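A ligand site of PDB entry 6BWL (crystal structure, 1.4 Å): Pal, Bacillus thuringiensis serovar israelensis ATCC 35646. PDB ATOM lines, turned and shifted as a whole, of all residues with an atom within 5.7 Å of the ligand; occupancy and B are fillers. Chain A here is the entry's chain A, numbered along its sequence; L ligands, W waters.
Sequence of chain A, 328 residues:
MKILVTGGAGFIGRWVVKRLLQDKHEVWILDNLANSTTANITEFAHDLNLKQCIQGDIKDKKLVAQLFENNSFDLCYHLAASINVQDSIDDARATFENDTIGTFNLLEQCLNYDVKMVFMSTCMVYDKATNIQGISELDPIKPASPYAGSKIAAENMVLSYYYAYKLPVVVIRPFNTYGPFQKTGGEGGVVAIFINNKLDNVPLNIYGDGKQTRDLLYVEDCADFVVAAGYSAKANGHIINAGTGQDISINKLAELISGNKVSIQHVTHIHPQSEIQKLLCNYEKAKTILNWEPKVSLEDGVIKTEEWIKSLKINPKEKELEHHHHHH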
ATOM      1  N   ILE A  83     -27.493 -23.061  26.520  1.00  0.00           N
ATOM      2  CA  ILE A  83     -26.949 -22.580  25.261  1.00  0.00           C
ATOM      3  C   ILE A  83     -27.500 -23.267  24.039  1.00  0.00           C
ATOM      4  O   ILE A  83     -27.118 -22.904  22.927  1.00  0.00           O
ATOM      5  CB  ILE A  83     -25.397 -22.675  25.243  1.00  0.00           C
ATOM      6  CG1 ILE A  83     -24.938 -24.121  25.254  1.00  0.00           C
ATOM      7  CG2 ILE A  83     -24.806 -21.923  26.445  1.00  0.00           C
ATOM      8  CD1 ILE A  83     -23.483 -24.344  24.847  1.00  0.00           C
ATOM      9  N   VAL A  85     -30.043 -24.292  21.195  1.00  0.00           N
ATOM     10  CA  VAL A  85     -31.242 -23.817  20.519  1.00  0.00           C
ATOM     11  C   VAL A  85     -32.351 -24.869  20.552  1.00  0.00           C
ATOM     12  O   VAL A  85     -33.493 -24.562  20.868  1.00  0.00           O
ATOM     13  CB  VAL A  85     -30.933 -23.341  19.094  1.00  0.00           C
ATOM     14  CG1 VAL A  85     -32.179 -23.082  18.255  1.00  0.00           C
ATOM     15  CG2 VAL A  85     -30.079 -22.076  19.113  1.00  0.00           C
ATOM     16  N   MET A 124     -26.638 -14.793  17.835  1.00  0.00           N
ATOM     17  CA  MET A 124     -27.869 -15.428  17.381  1.00  0.00           C
ATOM     18  C   MET A 124     -29.057 -14.470  17.489  1.00  0.00           C
ATOM     19  O   MET A 124     -30.076 -14.658  16.831  1.00  0.00           O
ATOM     20  CB  MET A 124     -28.144 -16.698  18.189  1.00  0.00           C
ATOM     21  CG  MET A 124     -27.055 -17.753  18.077  1.00  0.00           C
ATOM     22  SD  MET A 124     -26.807 -18.314  16.377  1.00  0.00           S
ATOM     23  CE  MET A 124     -28.215 -19.411  16.177  1.00  0.00           C
ATOM     24  N   ASN A 176     -20.356 -17.475  16.792  1.00  0.00           N
ATOM     25  CA  ASN A 176     -20.115 -18.879  17.074  1.00  0.00           C
ATOM     26  C   ASN A 176     -18.640 -19.125  17.352  1.00  0.00           C
ATOM     27  O   ASN A 176     -17.799 -18.801  16.538  1.00  0.00           O
ATOM     28  CB  ASN A 176     -20.531 -19.750  15.869  1.00  0.00           C
ATOM     29  CG  ASN A 176     -22.005 -19.744  15.622  1.00  0.00           C
ATOM     30  OD1 ASN A 176     -22.576 -18.701  15.347  1.00  0.00           O
ATOM     31  ND2 ASN A 176     -22.637 -20.909  15.740  1.00  0.00           N
ATOM     32  N   GLY A 188     -22.522 -30.436  21.668  1.00  0.00           N
ATOM     33  CA  GLY A 188     -21.394 -29.665  21.217  1.00  0.00           C
ATOM     34  C   GLY A 188     -21.701 -28.765  20.037  1.00  0.00           C
ATOM     35  O   GLY A 188     -22.831 -28.695  19.549  1.00  0.00           O
ATOM     36  N   GLY A 189     -20.686 -28.026  19.645  1.00  0.00           N
ATOM     37  CA  GLY A 189     -20.756 -27.161  18.471  1.00  0.00           C
ATOM     38  C   GLY A 189     -20.342 -27.925  17.249  1.00  0.00           C
ATOM     39  O   GLY A 189     -19.627 -28.937  17.327  1.00  0.00           O
ATOM     40  N   VAL A 190     -20.739 -27.389  16.091  1.00  0.00           N
ATOM     41  CA  VAL A 190     -20.520 -28.074  14.816  1.00  0.00           C
ATOM     42  C   VAL A 190     -19.053 -28.394  14.546  1.00  0.00           C
ATOM     43  O   VAL A 190     -18.765 -29.479  14.033  1.00  0.00           O
ATOM     44  CB  VAL A 190     -21.134 -27.268  13.648  1.00  0.00           C
ATOM     45  CG1 VAL A 190     -20.467 -25.924  13.398  1.00  0.00           C
ATOM     46  CG2 VAL A 190     -21.110 -28.114  12.387  1.00  0.00           C
ATOM     47  N   VAL A 191     -18.124 -27.530  14.903  1.00  0.00           N
ATOM     48  CA  VAL A 191     -16.735 -27.804  14.640  1.00  0.00           C
ATOM     49  C   VAL A 191     -16.275 -28.984  15.478  1.00  0.00           C
ATOM     50  O   VAL A 191     -15.607 -29.936  14.961  1.00  0.00           O
ATOM     51  CB  VAL A 191     -15.842 -26.583  14.921  1.00  0.00           C
ATOM     52  CG1 VAL A 191     -14.369 -26.966  14.783  1.00  0.00           C
ATOM     53  CG2 VAL A 191     -16.174 -25.433  13.991  1.00  0.00           C
ATOM     54  N   ILE A 193     -18.130 -31.393  16.827  1.00  0.00           N
ATOM     55  CA  ILE A 193     -18.847 -32.584  16.382  1.00  0.00           C
ATOM     56  C   ILE A 193     -18.197 -33.146  15.122  1.00  0.00           C
ATOM     57  O   ILE A 193     -17.905 -34.352  15.008  1.00  0.00           O
ATOM     58  CB  ILE A 193     -20.325 -32.298  16.141  1.00  0.00           C
ATOM     59  CG1 ILE A 193     -21.007 -32.049  17.497  1.00  0.00           C
ATOM     60  CG2 ILE A 193     -20.968 -33.462  15.404  1.00  0.00           C
ATOM     61  CD1 ILE A 193     -22.396 -31.453  17.392  1.00  0.00           C
ATOM     62  N   PHE A 194     -17.941 -32.295  14.152  1.00  0.00           N
ATOM     63  CA  PHE A 194     -17.351 -32.747  12.908  1.00  0.00           C
ATOM     64  C   PHE A 194     -15.927 -33.294  13.102  1.00  0.00           C
ATOM     65  O   PHE A 194     -15.588 -34.290  12.563  1.00  0.00           O
ATOM     66  CB  PHE A 194     -17.296 -31.590  11.907  1.00  0.00           C
ATOM     67  CG  PHE A 194     -18.615 -31.254  11.206  1.00  0.00           C
ATOM     68  CD1 PHE A 194     -18.652 -30.227  10.291  1.00  0.00           C
ATOM     69  CD2 PHE A 194     -19.740 -31.939  11.419  1.00  0.00           C
ATOM     70  CE1 PHE A 194     -19.805 -29.892   9.611  1.00  0.00           C
ATOM     71  CE2 PHE A 194     -20.914 -31.602  10.784  1.00  0.00           C
ATOM     72  CZ  PHE A 194     -20.949 -30.594   9.858  1.00  0.00           C
ATOM     73  N   ASN A 205     -22.730 -35.235   9.357  1.00  0.00           N
ATOM     74  CA  ASN A 205     -24.101 -35.023   8.953  1.00  0.00           C
ATOM     75  C   ASN A 205     -24.436 -33.546   9.020  1.00  0.00           C
ATOM     76  O   ASN A 205     -24.227 -32.882  10.060  1.00  0.00           O
ATOM     77  CB  ASN A 205     -25.067 -35.788   9.841  1.00  0.00           C
ATOM     78  CG  ASN A 205     -25.017 -37.281   9.636  1.00  0.00           C
ATOM     79  OD1 ASN A 205     -24.718 -37.774   8.554  1.00  0.00           O
ATOM     80  ND2 ASN A 205     -25.376 -38.022  10.648  1.00  0.00           N
ATOM     81  N   ILE A 206     -24.931 -33.034   7.917  1.00  0.00           N
ATOM     82  CA  ILE A 206     -25.271 -31.612   7.778  1.00  0.00           C
ATOM     83  C   ILE A 206     -26.752 -31.410   7.787  1.00  0.00           C
ATOM     84  O   ILE A 206     -27.509 -32.057   7.043  1.00  0.00           O
ATOM     85  CB  ILE A 206     -24.725 -31.076   6.445  1.00  0.00           C
ATOM     86  CG1 ILE A 206     -23.192 -31.210   6.420  1.00  0.00           C
ATOM     87  CG2 ILE A 206     -25.182 -29.665   6.180  1.00  0.00           C
ATOM     88  CD1 ILE A 206     -22.593 -30.850   5.075  1.00  0.00           C
ATOM     89  N   TYR A 207     -27.200 -30.517   8.668  1.00  0.00           N
ATOM     90  CA  TYR A 207     -28.637 -30.199   8.763  1.00  0.00           C
ATOM     91  C   TYR A 207     -29.067 -29.303   7.594  1.00  0.00           C
ATOM     92  O   TYR A 207     -28.457 -28.298   7.259  1.00  0.00           O
ATOM     93  CB  TYR A 207     -28.898 -29.462  10.084  1.00  0.00           C
ATOM     94  CG  TYR A 207     -28.853 -30.313  11.308  1.00  0.00           C
ATOM     95  CD1 TYR A 207     -28.023 -29.998  12.372  1.00  0.00           C
ATOM     96  CD2 TYR A 207     -29.609 -31.461  11.427  1.00  0.00           C
ATOM     97  CE1 TYR A 207     -27.997 -30.790  13.495  1.00  0.00           C
ATOM     98  CE2 TYR A 207     -29.591 -32.249  12.550  1.00  0.00           C
ATOM     99  CZ  TYR A 207     -28.773 -31.910  13.589  1.00  0.00           C
ATOM    100  OH  TYR A 207     -28.762 -32.710  14.715  1.00  0.00           O
ATOM    101  N   GLN A 212     -26.329 -22.643   4.751  1.00  0.00           N
ATOM    102  CA  GLN A 212     -26.297 -21.670   5.829  1.00  0.00           C
ATOM    103  C   GLN A 212     -24.843 -21.438   6.234  1.00  0.00           C
ATOM    104  O   GLN A 212     -24.018 -22.371   6.211  1.00  0.00           O
ATOM    105  CB  GLN A 212     -27.134 -22.116   7.029  1.00  0.00           C
ATOM    106  CG  GLN A 212     -26.674 -23.365   7.799  1.00  0.00           C
ATOM    107  CD  GLN A 212     -27.201 -24.694   7.295  1.00  0.00           C
ATOM    108  OE1 GLN A 212     -27.506 -24.844   6.116  1.00  0.00           O
ATOM    109  NE2 GLN A 212     -27.336 -25.663   8.187  1.00  0.00           N
ATOM    110  N   ARG A 214     -21.675 -19.641   8.829  1.00  0.00           N
ATOM    111  CA  ARG A 214     -21.231 -19.191  10.127  1.00  0.00           C
ATOM    112  C   ARG A 214     -19.910 -18.465  10.055  1.00  0.00           C
ATOM    113  O   ARG A 214     -19.041 -18.801   9.243  1.00  0.00           O
ATOM    114  CB  ARG A 214     -21.127 -20.360  11.117  1.00  0.00           C
ATOM    115  CG  ARG A 214     -22.399 -21.082  11.485  1.00  0.00           C
ATOM    116  CD  ARG A 214     -23.344 -20.141  12.222  1.00  0.00           C
ATOM    117  NE  ARG A 214     -24.541 -20.775  12.728  1.00  0.00           N
ATOM    118  CZ  ARG A 214     -25.730 -20.785  12.136  1.00  0.00           C
ATOM    119  NH1 ARG A 214     -25.901 -20.307  10.932  1.00  0.00           N
ATOM    120  NH2 ARG A 214     -26.751 -21.279  12.791  1.00  0.00           N
ATOM    121  N   ILE A 250     -21.815 -24.447   5.942  1.00  0.00           N
ATOM    122  CA  ILE A 250     -21.630 -25.721   6.632  1.00  0.00           C
ATOM    123  C   ILE A 250     -21.152 -26.783   5.639  1.00  0.00           C
ATOM    124  O   ILE A 250     -20.281 -27.583   5.993  1.00  0.00           O
ATOM    125  CB  ILE A 250     -22.856 -26.140   7.473  1.00  0.00           C
ATOM    126  CG1 ILE A 250     -23.250 -25.012   8.470  1.00  0.00           C
ATOM    127  CG2 ILE A 250     -22.584 -27.439   8.195  1.00  0.00           C
ATOM    128  CD1 ILE A 250     -22.139 -24.557   9.372  1.00  0.00           C
ATOM    129  N   HIS A 269     -33.246 -30.866   8.628  1.00  0.00           N
ATOM    130  CA  HIS A 269     -32.901 -29.829   9.590  1.00  0.00           C
ATOM    131  C   HIS A 269     -33.763 -29.972  10.830  1.00  0.00           C
ATOM    132  O   HIS A 269     -34.993 -30.132  10.739  1.00  0.00           O
ATOM    133  CB  HIS A 269     -33.067 -28.446   8.975  1.00  0.00           C
ATOM    134  CG  HIS A 269     -32.257 -27.394   9.650  1.00  0.00           C
ATOM    135  ND1 HIS A 269     -32.432 -27.045  10.967  1.00  0.00           N
ATOM    136  CD2 HIS A 269     -31.277 -26.610   9.167  1.00  0.00           C
ATOM    137  CE1 HIS A 269     -31.562 -26.092  11.279  1.00  0.00           C
ATOM    138  NE2 HIS A 269     -30.858 -25.798  10.201  1.00  0.00           N
ATOM    139  N   HIS A 271     -34.390 -27.661  13.110  1.00  0.00           N
ATOM    140  CA  HIS A 271     -35.159 -26.442  13.392  1.00  0.00           C
ATOM    141  C   HIS A 271     -34.967 -25.391  12.324  1.00  0.00           C
ATOM    142  O   HIS A 271     -34.460 -24.293  12.580  1.00  0.00           O
ATOM    143  CB  HIS A 271     -34.864 -25.888  14.788  1.00  0.00           C
ATOM    144  CG  HIS A 271     -33.416 -25.714  15.130  1.00  0.00           C
ATOM    145  ND1 HIS A 271     -32.840 -26.456  16.133  1.00  0.00           N
ATOM    146  CD2 HIS A 271     -32.493 -24.793  14.767  1.00  0.00           C
ATOM    147  CE1 HIS A 271     -31.595 -26.072  16.309  1.00  0.00           C
ATOM    148  NE2 HIS A 271     -31.357 -25.072  15.490  1.00  0.00           N
ATOM    149  N   GLU A 275     -33.367 -21.249  12.201  1.00  0.00           N
ATOM    150  CA  GLU A 275     -32.055 -21.103  11.612  1.00  0.00           C
ATOM    151  C   GLU A 275     -31.790 -19.651  11.221  1.00  0.00           C
ATOM    152  O   GLU A 275     -32.740 -18.861  11.034  1.00  0.00           O
ATOM    153  CB  GLU A 275     -31.937 -22.060  10.403  1.00  0.00           C
ATOM    154  CG  GLU A 275     -30.599 -22.119   9.679  1.00  0.00           C
ATOM    155  CD  GLU A 275     -29.461 -22.519  10.593  1.00  0.00           C
ATOM    156  OE1 GLU A 275     -29.011 -21.658  11.387  1.00  0.00           O
ATOM    157  OE2 GLU A 275     -29.010 -23.696  10.591  1.00  0.00           O
ATOM    158  N   LEU A 279     -24.600 -15.751   8.907  1.00  0.00           N
ATOM    159  CA  LEU A 279     -24.004 -15.083  10.057  1.00  0.00           C
ATOM    160  C   LEU A 279     -22.593 -14.636   9.699  1.00  0.00           C
ATOM    161  O   LEU A 279     -21.692 -15.446   9.398  1.00  0.00           O
ATOM    162  CB  LEU A 279     -24.005 -15.963  11.311  1.00  0.00           C
ATOM    163  CG  LEU A 279     -25.321 -16.025  12.075  1.00  0.00           C
ATOM    164  CD1 LEU A 279     -25.378 -17.187  13.048  1.00  0.00           C
ATOM    165  CD2 LEU A 279     -25.620 -14.706  12.781  1.00  0.00           C
HETATM  166  N1  LIG L   1     -24.812 -28.309  12.062  1.00  0.00           N
HETATM  167  C1  LIG L   1     -24.718 -29.399  11.164  1.00  0.00           C
HETATM  168  N2  LIG L   1     -24.415 -30.576  11.656  1.00  0.00           N
HETATM  169  C2  LIG L   1     -24.131 -30.836  12.945  1.00  0.00           C
HETATM  170  C3  LIG L   1     -24.218 -29.780  13.848  1.00  0.00           C
HETATM  171  C4  LIG L   1     -24.551 -28.547  13.371  1.00  0.00           C
HETATM  172  O1  LIG L   1     -24.991 -29.167   9.958  1.00  0.00           O
HETATM  173  O2  LIG L   1     -23.834 -31.999  13.335  1.00  0.00           O
HETATM  174  C5  LIG L   1     -25.109 -26.975  11.574  1.00  0.00           C
HETATM  175  C6  LIG L   1     -26.303 -26.310  12.225  1.00  0.00           C
HETATM  176  O3  LIG L   1     -27.473 -26.684  11.516  1.00  0.00           O
HETATM  177  C7  LIG L   1     -25.979 -24.834  12.170  1.00  0.00           C
HETATM  178  C8  LIG L   1     -24.449 -24.787  12.260  1.00  0.00           C
HETATM  179  O4  LIG L   1     -24.019 -26.118  11.911  1.00  0.00           O
HETATM  180  O5  LIG L   1     -26.387 -24.270  10.894  1.00  0.00           O
HETATM  181  C9  LIG L   1     -23.901 -24.447  13.639  1.00  0.00           C
HETATM  182  O6  LIG L   1     -24.597 -25.272  14.564  1.00  0.00           O
HETATM  183  P1  LIG L   1     -24.229 -25.259  16.111  1.00  0.00           P
HETATM  184  O7  LIG L   1     -25.144 -26.220  16.767  1.00  0.00           O
HETATM  185  O8  LIG L   1     -22.737 -25.345  16.276  1.00  0.00           O
HETATM  186  O9  LIG L   1     -24.584 -23.795  16.663  1.00  0.00           O
HETATM  187  P2  LIG L   1     -25.797 -22.736  16.390  1.00  0.00           P
HETATM  188  O10 LIG L   1     -27.031 -23.470  15.946  1.00  0.00           O
HETATM  189  O11 LIG L   1     -25.624 -21.987  17.693  1.00  0.00           O
HETATM  190  O12 LIG L   1     -25.433 -21.838  15.346  1.00  0.00           O
HETATM  191  O   HOH W   1     -24.874 -33.607  15.334  1.00  0.00           O
HETATM  192  O   HOH W   2     -27.330 -27.546  15.572  1.00  0.00           O
HETATM  193  O   HOH W   3     -21.153 -23.294  16.718  1.00  0.00           O
HETATM  194  O   HOH W   4     -26.534 -21.424  19.953  1.00  0.00           O
HETATM  195  O   HOH W   5     -28.646 -25.264  16.644  1.00  0.00           O
HETATM  196  O   HOH W   6     -26.348 -26.588  19.107  1.00  0.00           O
HETATM  197  O   HOH W   7     -29.227 -26.799  13.511  1.00  0.00           O
HETATM  198  O   HOH W   8     -24.177 -28.751  17.094  1.00  0.00           O
HETATM  199  O   HOH W   9     -22.465 -34.572  12.189  1.00  0.00           O
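OE1 of Glu 275 lies within salt-bridge range of NH2 of Arg 214. A ring nitrogen (NE2) of His 269 lies within hydrogen-bond range of the side-chain carboxylate of Glu 275 (2.8 Å). NE2 of Gln 212 sits at hydrogen-bond distance from O of Tyr 207, at 3.0 Å. The backbone carbonyl oxygen of Gln 212 sits at hydrogen-bond distance from the backbone NH of Ile 250 (3.0 Å). A ring nitrogen (ND1) of His 269 lies within hydrogen-bond range of the backbone NH (N) of His 271 (3.0 Å).
Water W4 bridges an oxygen (O11) of the ligand (2.5 Å) and the backbone carbonyl oxygen of Ile 83 (3.4 Å). Water W5 bridges an oxygen (O10) of the ligand (2.5 Å) and a ring nitrogen (NE2) of His 271 (3.0 Å). Water W3 bridges an oxygen (O8) of the ligand and the side-chain amide nitrogen of Asn 176. Water W7 bridges O3 of the ligand (2.7 Å) and NE2 of His 271 (3.4 Å). Water W8 bridges an oxygen (O7) of the ligand (2.7 Å) and the backbone carbonyl oxygen of Gly 188 (2.8 Å). Water W9 lies within hydrogen-bond range of the backbone NH of Asn 205 (2.9 Å) and an oxygen (O2) of the ligand (3.1 Å).
An oxygen (O5) of the ligand is in hydrogen-bond range of the side-chain carboxylate (OE2) of Glu 275 (2.7 Å). The backbone carbonyl oxygen of Asn 205 sits at hydrogen-bond distance from a nitrogen (N2) of the ligand (2.8 Å). The backbone NH (N) of Val 190 sits at hydrogen-bond distance from an oxygen (O8) of the ligand (2.9 Å). An oxygen (O1) of the ligand is in hydrogen-bond range of the backbone NH (N) of Tyr 207 (2.9 Å). The guanidinium group of Arg 214 lies within salt-bridge range of an oxygen (O12) of the ligand. The side-chain amide nitrogen (ND2) of Asn 176 is in hydrogen-bond range of an oxygen (O12) of the ligand (3.0 Å). NE2 of Gln 212 sits at hydrogen-bond distance from O5 of the ligand, 3.2 Å away.
Merely in contact with the ligand: Met 124, Gly 189, Ile 193, Phe 194, Ile 206, Ile 250 and His 269. Hydrophobic or aromatic side chains that line the ligand: Met 124, Val 190, Ile 193, Phe 194, Ile 206, Tyr 207 and Ile 250. 14 residues have an atom within 4 Å of the ligand: Met 124, Asn 176, Gly 189, Val 190, Ile 193, Phe 194, Asn 205, Ile 206, Tyr 207, Gln 212, Arg 214, Ile 250, His 269 and Glu 275. The nearest printed residue that does not touch the ligand is Gly 188 (4.4 Å).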
